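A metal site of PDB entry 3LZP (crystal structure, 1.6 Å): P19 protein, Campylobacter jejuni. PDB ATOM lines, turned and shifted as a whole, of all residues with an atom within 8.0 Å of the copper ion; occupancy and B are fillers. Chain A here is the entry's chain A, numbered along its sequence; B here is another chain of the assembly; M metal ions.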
ATOM      1  N   LEU A  22       5.245  -6.844  -4.681  1.00  0.00           N
ATOM      2  CA  LEU A  22       4.346  -6.340  -5.714  1.00  0.00           C
ATOM      3  C   LEU A  22       4.076  -7.441  -6.715  1.00  0.00           C
ATOM      4  O   LEU A  22       4.507  -8.563  -6.509  1.00  0.00           O
ATOM      5  CB  LEU A  22       4.893  -5.088  -6.380  1.00  0.00           C
ATOM      6  CG  LEU A  22       6.301  -4.991  -6.949  1.00  0.00           C
ATOM      7  CD1 LEU A  22       6.335  -3.792  -7.912  1.00  0.00           C
ATOM      8  CD2 LEU A  22       7.347  -4.789  -5.851  1.00  0.00           C
ATOM      9  N   GLN A  23       3.351  -7.120  -7.788  1.00  0.00           N
ATOM     10  CA  GLN A  23       3.162  -8.049  -8.895  1.00  0.00           C
ATOM     11  C   GLN A  23       4.502  -8.524  -9.434  1.00  0.00           C
ATOM     12  O   GLN A  23       5.504  -7.793  -9.301  1.00  0.00           O
ATOM     13  CB  GLN A  23       2.354  -7.391 -10.036  1.00  0.00           C
ATOM     14  CG  GLN A  23       3.060  -6.295 -10.840  1.00  0.00           C
ATOM     15  CD  GLN A  23       2.909  -4.898 -10.266  1.00  0.00           C
ATOM     16  OE1 GLN A  23       2.559  -4.728  -9.073  1.00  0.00           O
ATOM     17  NE2 GLN A  23       3.141  -3.873 -11.110  1.00  0.00           N
ATOM     18  N   ILE A  25       7.513  -8.915 -11.921  1.00  0.00           N
ATOM     19  CA  ILE A  25       8.061  -7.885 -12.807  1.00  0.00           C
ATOM     20  C   ILE A  25       8.824  -8.586 -13.933  1.00  0.00           C
ATOM     21  O   ILE A  25       9.349  -9.692 -13.759  1.00  0.00           O
ATOM     22  CB  ILE A  25       8.948  -6.931 -11.965  1.00  0.00           C
ATOM     23  CG1 ILE A  25       8.044  -6.039 -11.096  1.00  0.00           C
ATOM     24  CG2 ILE A  25       9.890  -6.117 -12.840  1.00  0.00           C
ATOM     25  CD1 ILE A  25       7.137  -5.123 -11.831  1.00  0.00           C
ATOM     26  N   GLU A  26       8.853  -7.986 -15.108  1.00  0.00           N
ATOM     27  CA  GLU A  26       9.678  -8.498 -16.185  1.00  0.00           C
ATOM     28  C   GLU A  26      11.024  -7.798 -16.049  1.00  0.00           C
ATOM     29  O   GLU A  26      11.057  -6.562 -15.940  1.00  0.00           O
ATOM     30  CB  GLU A  26       9.046  -8.202 -17.544  1.00  0.00           C
ATOM     31  CG  GLU A  26       9.183  -9.268 -18.568  1.00  0.00           C
ATOM     32  CD  GLU A  26       8.463 -10.525 -18.182  1.00  0.00           C
ATOM     33  OE1 GLU A  26       7.218 -10.580 -18.380  1.00  0.00           O
ATOM     34  OE2 GLU A  26       9.137 -11.455 -17.679  1.00  0.00           O
ATOM     35  N   MET A  27      12.117  -8.548 -16.009  1.00  0.00           N
ATOM     36  CA  MET A  27      13.424  -7.971 -15.751  1.00  0.00           C
ATOM     37  C   MET A  27      14.386  -8.332 -16.862  1.00  0.00           C
ATOM     38  O   MET A  27      14.320  -9.422 -17.375  1.00  0.00           O
ATOM     39  CB  MET A  27      14.021  -8.498 -14.446  1.00  0.00           C
ATOM     40  CG  MET A  27      15.253  -7.740 -13.909  1.00  0.00           C
ATOM     41  SD  MET A  27      16.183  -8.613 -12.620  1.00  0.00           S
ATOM     42  CE  MET A  27      17.177  -9.741 -13.630  1.00  0.00           C
ATOM     43  N   ASP A  33      16.679 -14.090 -13.633  1.00  0.00           N
ATOM     44  CA  ASP A  33      15.602 -14.297 -12.668  1.00  0.00           C
ATOM     45  C   ASP A  33      14.364 -14.945 -13.261  1.00  0.00           C
ATOM     46  O   ASP A  33      14.140 -14.919 -14.471  1.00  0.00           O
ATOM     47  CB  ASP A  33      15.177 -12.993 -11.980  1.00  0.00           C
ATOM     48  CG  ASP A  33      14.516 -13.234 -10.607  1.00  0.00           C
ATOM     49  OD1 ASP A  33      14.741 -14.299  -9.978  1.00  0.00           O
ATOM     50  OD2 ASP A  33      13.769 -12.359 -10.154  1.00  0.00           O
ATOM     51  N   HIS A  42       6.841 -10.129  -6.775  1.00  0.00           N
ATOM     52  CA  HIS A  42       8.213  -9.622  -6.780  1.00  0.00           C
ATOM     53  C   HIS A  42       8.466  -9.178  -5.355  1.00  0.00           C
ATOM     54  O   HIS A  42       7.743  -8.309  -4.824  1.00  0.00           O
ATOM     55  CB  HIS A  42       8.381  -8.445  -7.741  1.00  0.00           C
ATOM     56  CG  HIS A  42       9.827  -8.083  -8.034  1.00  0.00           C
ATOM     57  ND1 HIS A  42      10.656  -8.909  -8.759  1.00  0.00           N
ATOM     58  CD2 HIS A  42      10.536  -6.957  -7.777  1.00  0.00           C
ATOM     59  CE1 HIS A  42      11.827  -8.308  -8.936  1.00  0.00           C
ATOM     60  NE2 HIS A  42      11.785  -7.145  -8.315  1.00  0.00           N
ATOM     61  N   LEU A  43       9.459  -9.801  -4.722  1.00  0.00           N
ATOM     62  CA  LEU A  43       9.846  -9.480  -3.350  1.00  0.00           C
ATOM     63  C   LEU A  43      10.993  -8.491  -3.409  1.00  0.00           C
ATOM     64  O   LEU A  43      11.943  -8.684  -4.189  1.00  0.00           O
ATOM     65  CB  LEU A  43      10.253 -10.751  -2.620  1.00  0.00           C
ATOM     66  CG  LEU A  43      10.769 -10.654  -1.182  1.00  0.00           C
ATOM     67  CD1 LEU A  43       9.723 -10.049  -0.264  1.00  0.00           C
ATOM     68  CD2 LEU A  43      11.201 -12.052  -0.652  1.00  0.00           C
ATOM     69  N   GLU A  44      10.914  -7.458  -2.595  1.00  0.00           N
ATOM     70  CA  GLU A  44      11.988  -6.417  -2.572  1.00  0.00           C
ATOM     71  C   GLU A  44      12.423  -6.143  -1.157  1.00  0.00           C
ATOM     72  O   GLU A  44      11.594  -6.113  -0.248  1.00  0.00           O
ATOM     73  CB  GLU A  44      11.503  -5.115  -3.179  1.00  0.00           C
ATOM     74  CG  GLU A  44      10.983  -5.241  -4.598  1.00  0.00           C
ATOM     75  CD  GLU A  44      10.817  -3.885  -5.256  1.00  0.00           C
ATOM     76  OE1 GLU A  44      10.866  -2.894  -4.511  1.00  0.00           O
ATOM     77  OE2 GLU A  44      10.622  -3.836  -6.500  1.00  0.00           O
ATOM     78  N   ALA A  45      13.718  -5.895  -1.000  1.00  0.00           N
ATOM     79  CA  ALA A  45      14.251  -5.294   0.201  1.00  0.00           C
ATOM     80  C   ALA A  45      14.577  -3.872  -0.177  1.00  0.00           C
ATOM     81  O   ALA A  45      15.262  -3.638  -1.159  1.00  0.00           O
ATOM     82  CB  ALA A  45      15.521  -5.983   0.674  1.00  0.00           C
ATOM     83  N   MET A  86      18.472  -9.840  -5.832  1.00  0.00           N
ATOM     84  CA  MET A  86      19.513  -9.322  -6.691  1.00  0.00           C
ATOM     85  C   MET A  86      19.363  -7.798  -6.870  1.00  0.00           C
ATOM     86  O   MET A  86      18.237  -7.259  -6.822  1.00  0.00           O
ATOM     87  CB  MET A  86      19.507 -10.058  -8.038  1.00  0.00           C
ATOM     88  CG  MET A  86      18.302  -9.866  -8.899  1.00  0.00           C
ATOM     89  SD  MET A  86      18.642 -10.436 -10.580  1.00  0.00           S
ATOM     90  CE  MET A  86      19.637  -9.071 -11.201  1.00  0.00           C
ATOM     91  N   PRO A  87      20.491  -7.094  -7.038  1.00  0.00           N
ATOM     92  CA  PRO A  87      20.352  -5.659  -7.212  1.00  0.00           C
ATOM     93  C   PRO A  87      19.800  -5.308  -8.600  1.00  0.00           C
ATOM     94  O   PRO A  87      20.122  -5.987  -9.575  1.00  0.00           O
ATOM     95  CB  PRO A  87      21.775  -5.171  -7.083  1.00  0.00           C
ATOM     96  CG  PRO A  87      22.583  -6.291  -7.463  1.00  0.00           C
ATOM     97  CD  PRO A  87      21.903  -7.507  -7.110  1.00  0.00           C
ATOM     98  N   MET A  88      18.941  -4.297  -8.672  1.00  0.00           N
ATOM     99  CA  MET A  88      18.336  -3.899  -9.940  1.00  0.00           C
ATOM    100  C   MET A  88      17.667  -2.526  -9.742  1.00  0.00           C
ATOM    101  O   MET A  88      17.568  -2.055  -8.632  1.00  0.00           O
ATOM    102  CB  MET A  88      17.258  -4.930 -10.366  1.00  0.00           C
ATOM    103  CG  MET A  88      16.056  -4.870  -9.506  1.00  0.00           C
ATOM    104  SD  MET A  88      14.922  -6.193  -9.884  1.00  0.00           S
ATOM    105  CE  MET A  88      15.804  -7.560  -9.110  1.00  0.00           C
ATOM    106  N   VAL A  89      17.217  -1.931 -10.832  1.00  0.00           N
ATOM    107  CA  VAL A  89      16.619  -0.608 -10.827  1.00  0.00           C
ATOM    108  C   VAL A  89      15.246  -0.640 -11.502  1.00  0.00           C
ATOM    109  O   VAL A  89      14.981  -1.381 -12.502  1.00  0.00           O
ATOM    110  CB  VAL A  89      17.541   0.462 -11.459  1.00  0.00           C
ATOM    111  CG1 VAL A  89      17.690   0.280 -13.020  1.00  0.00           C
ATOM    112  CG2 VAL A  89      17.042   1.892 -11.121  1.00  0.00           C
ATOM    113  N   ALA A  90      14.303   0.052 -10.857  1.00  0.00           N
ATOM    114  CA  ALA A  90      12.997   0.286 -11.411  1.00  0.00           C
ATOM    115  C   ALA A  90      12.788   1.794 -11.573  1.00  0.00           C
ATOM    116  O   ALA A  90      13.721   2.589 -11.348  1.00  0.00           O
ATOM    117  CB  ALA A  90      11.872  -0.394 -10.536  1.00  0.00           C
ATOM    118  N   GLY A  93      13.752   3.819  -8.614  1.00  0.00           N
ATOM    119  CA  GLY A  93      15.093   3.693  -8.082  1.00  0.00           C
ATOM    120  C   GLY A  93      15.571   2.264  -7.842  1.00  0.00           C
ATOM    121  O   GLY A  93      14.844   1.301  -8.060  1.00  0.00           O
ATOM    122  N   PRO A  94      16.813   2.131  -7.377  1.00  0.00           N
ATOM    123  CA  PRO A  94      17.405   0.801  -7.159  1.00  0.00           C
ATOM    124  C   PRO A  94      16.835   0.100  -5.946  1.00  0.00           C
ATOM    125  O   PRO A  94      16.391   0.740  -4.996  1.00  0.00           O
ATOM    126  CB  PRO A  94      18.886   1.087  -6.934  1.00  0.00           C
ATOM    127  CG  PRO A  94      18.911   2.569  -6.432  1.00  0.00           C
ATOM    128  CD  PRO A  94      17.774   3.239  -7.124  1.00  0.00           C
ATOM    129  N   HIS A  95      16.806  -1.225  -5.988  1.00  0.00           N
ATOM    130  CA  HIS A  95      16.392  -2.053  -4.870  1.00  0.00           C
ATOM    131  C   HIS A  95      17.005  -3.443  -5.031  1.00  0.00           C
ATOM    132  O   HIS A  95      17.790  -3.687  -5.972  1.00  0.00           O
ATOM    133  CB  HIS A  95      14.861  -2.114  -4.758  1.00  0.00           C
ATOM    134  CG  HIS A  95      14.202  -2.760  -5.954  1.00  0.00           C
ATOM    135  ND1 HIS A  95      13.583  -2.014  -6.925  1.00  0.00           N
ATOM    136  CD2 HIS A  95      14.119  -4.042  -6.350  1.00  0.00           C
ATOM    137  CE1 HIS A  95      13.131  -2.808  -7.881  1.00  0.00           C
ATOM    138  NE2 HIS A  95      13.428  -4.053  -7.550  1.00  0.00           N
ATOM    139  N   TYR A  96      16.740  -4.325  -4.067  1.00  0.00           N
ATOM    140  CA  TYR A  96      17.153  -5.694  -4.169  1.00  0.00           C
ATOM    141  C   TYR A  96      15.851  -6.497  -4.305  1.00  0.00           C
ATOM    142  O   TYR A  96      14.883  -6.248  -3.581  1.00  0.00           O
ATOM    143  CB  TYR A  96      17.933  -6.180  -2.928  1.00  0.00           C
ATOM    144  CG  TYR A  96      19.259  -5.491  -2.708  1.00  0.00           C
ATOM    145  CD1 TYR A  96      20.415  -5.955  -3.324  1.00  0.00           C
ATOM    146  CD2 TYR A  96      19.344  -4.342  -1.893  1.00  0.00           C
ATOM    147  CE1 TYR A  96      21.619  -5.282  -3.119  1.00  0.00           C
ATOM    148  CE2 TYR A  96      20.545  -3.699  -1.658  1.00  0.00           C
ATOM    149  CZ  TYR A  96      21.661  -4.139  -2.288  1.00  0.00           C
ATOM    150  OH  TYR A  96      22.882  -3.499  -2.116  1.00  0.00           O
ATOM    151  N   GLY A  97      15.796  -7.405  -5.278  1.00  0.00           N
ATOM    152  CA  GLY A  97      14.501  -8.065  -5.581  1.00  0.00           C
ATOM    153  C   GLY A  97      14.628  -9.434  -6.211  1.00  0.00           C
ATOM    154  O   GLY A  97      15.715  -9.833  -6.643  1.00  0.00           O
ATOM    155  N   ALA A  98      13.510 -10.133  -6.236  1.00  0.00           N
ATOM    156  CA  ALA A  98      13.380 -11.425  -6.889  1.00  0.00           C
ATOM    157  C   ALA A  98      11.896 -11.718  -7.185  1.00  0.00           C
ATOM    158  O   ALA A  98      11.037 -11.472  -6.354  1.00  0.00           O
ATOM    159  CB  ALA A  98      13.949 -12.530  -5.994  1.00  0.00           C
ATOM    160  N   ASN A  99      11.619 -12.252  -8.378  1.00  0.00           N
ATOM    161  CA  ASN A  99      10.334 -12.848  -8.660  1.00  0.00           C
ATOM    162  C   ASN A  99      10.220 -14.187  -7.944  1.00  0.00           C
ATOM    163  O   ASN A  99      11.174 -15.008  -7.949  1.00  0.00           O
ATOM    164  CB  ASN A  99      10.186 -13.047 -10.171  1.00  0.00           C
ATOM    165  CG  ASN A  99       9.637 -11.832 -10.894  1.00  0.00           C
ATOM    166  OD1 ASN A  99       9.211 -10.853 -10.288  1.00  0.00           O
ATOM    167  ND2 ASN A  99       9.605 -11.919 -12.225  1.00  0.00           N
ATOM    168  N   GLY B 130      20.291  -5.775 -12.619  1.00  0.00           N
ATOM    169  CA  GLY B 130      19.123  -5.822 -13.474  1.00  0.00           C
ATOM    170  C   GLY B 130      18.327  -4.535 -13.625  1.00  0.00           C
ATOM    171  O   GLY B 130      18.574  -3.529 -12.947  1.00  0.00           O
ATOM    172  N   ARG B 131      17.346  -4.579 -14.505  1.00  0.00           N
ATOM    173  CA  ARG B 131      16.402  -3.463 -14.622  1.00  0.00           C
ATOM    174  C   ARG B 131      14.997  -3.989 -14.926  1.00  0.00           C
ATOM    175  O   ARG B 131      14.854  -4.967 -15.688  1.00  0.00           O
ATOM    176  CB  ARG B 131      16.853  -2.440 -15.667  1.00  0.00           C
ATOM    177  CG  ARG B 131      16.867  -2.920 -17.058  1.00  0.00           C
ATOM    178  CD  ARG B 131      17.342  -1.867 -18.035  1.00  0.00           C
ATOM    179  NE  ARG B 131      17.446  -2.541 -19.324  1.00  0.00           N
ATOM    180  CZ  ARG B 131      16.571  -2.455 -20.324  1.00  0.00           C
ATOM    181  NH1 ARG B 131      15.531  -1.615 -20.327  1.00  0.00           N
ATOM    182  NH2 ARG B 131      16.808  -3.188 -21.401  1.00  0.00           N
ATOM    183  N   HIS B 132      13.972  -3.352 -14.363  1.00  0.00           N
ATOM    184  CA  HIS B 132      12.581  -3.664 -14.692  1.00  0.00           C
ATOM    185  C   HIS B 132      12.309  -3.142 -16.111  1.00  0.00           C
ATOM    186  O   HIS B 132      12.845  -2.062 -16.499  1.00  0.00           O
ATOM    187  CB  HIS B 132      11.648  -2.969 -13.725  1.00  0.00           C
ATOM    188  CG  HIS B 132      11.677  -3.511 -12.334  1.00  0.00           C
ATOM    189  ND1 HIS B 132      10.605  -3.393 -11.469  1.00  0.00           N
ATOM    190  CD2 HIS B 132      12.622  -4.225 -11.688  1.00  0.00           C
ATOM    191  CE1 HIS B 132      10.913  -4.001 -10.330  1.00  0.00           C
ATOM    192  NE2 HIS B 132      12.153  -4.485 -10.433  1.00  0.00           N
ATOM    193  N   ASP B 134       8.888  -3.850 -17.383  1.00  0.00           N
ATOM    194  CA  ASP B 134       7.406  -3.949 -17.490  1.00  0.00           C
ATOM    195  C   ASP B 134       6.864  -2.550 -17.722  1.00  0.00           C
ATOM    196  O   ASP B 134       7.557  -1.580 -17.449  1.00  0.00           O
ATOM    197  CB  ASP B 134       6.807  -4.542 -16.229  1.00  0.00           C
ATOM    198  CG  ASP B 134       7.233  -3.788 -14.988  1.00  0.00           C
ATOM    199  OD1 ASP B 134       8.461  -3.816 -14.679  1.00  0.00           O
ATOM    200  OD2 ASP B 134       6.380  -3.144 -14.357  1.00  0.00           O
ATOM    201  N   THR B 137       6.546  -0.215 -14.126  1.00  0.00           N
ATOM    202  CA  THR B 137       7.741   0.181 -13.354  1.00  0.00           C
ATOM    203  C   THR B 137       9.054   0.147 -14.138  1.00  0.00           C
ATOM    204  O   THR B 137      10.148   0.371 -13.560  1.00  0.00           O
ATOM    205  CB  THR B 137       7.900  -0.714 -12.114  1.00  0.00           C
ATOM    206  OG1 THR B 137       8.336  -2.021 -12.511  1.00  0.00           O
ATOM    207  CG2 THR B 137       6.605  -0.800 -11.328  1.00  0.00           C
HETATM  208 CU    CU M   1      12.949  -5.592  -8.801  1.00  0.00          CU
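The backbone NH (N) of His 42 is in hydrogen-bond range of the backbone carbonyl oxygen (O) of Leu 22 (2.8 Å). ND1 of His 42 is in hydrogen-bond range of OD1 of Asn 99 (2.9 Å). NE2 of His 95 lies close to OE2 of Glu 44 (3.0 Å). N of His 132 of chain B lies within hydrogen-bond range of O of Val 89, 2.9 Å away. ND1 of His 132 of chain B is in hydrogen-bond range of OG1 of Thr 137 of chain B (2.8 Å).
Glu 44 touches the copper ion. The nearest printed residue that does not touch the copper ion is Gly 97 (4.3 Å).
The copper ion is bound by NE2 of His 42 (2.0 Å), NE2 of His 95 (2.0 Å), NE2 of His 132 of chain B (2.1 Å) and SD of Met 88 (2.3 Å). The copper ion has four donor atoms within binding distance.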
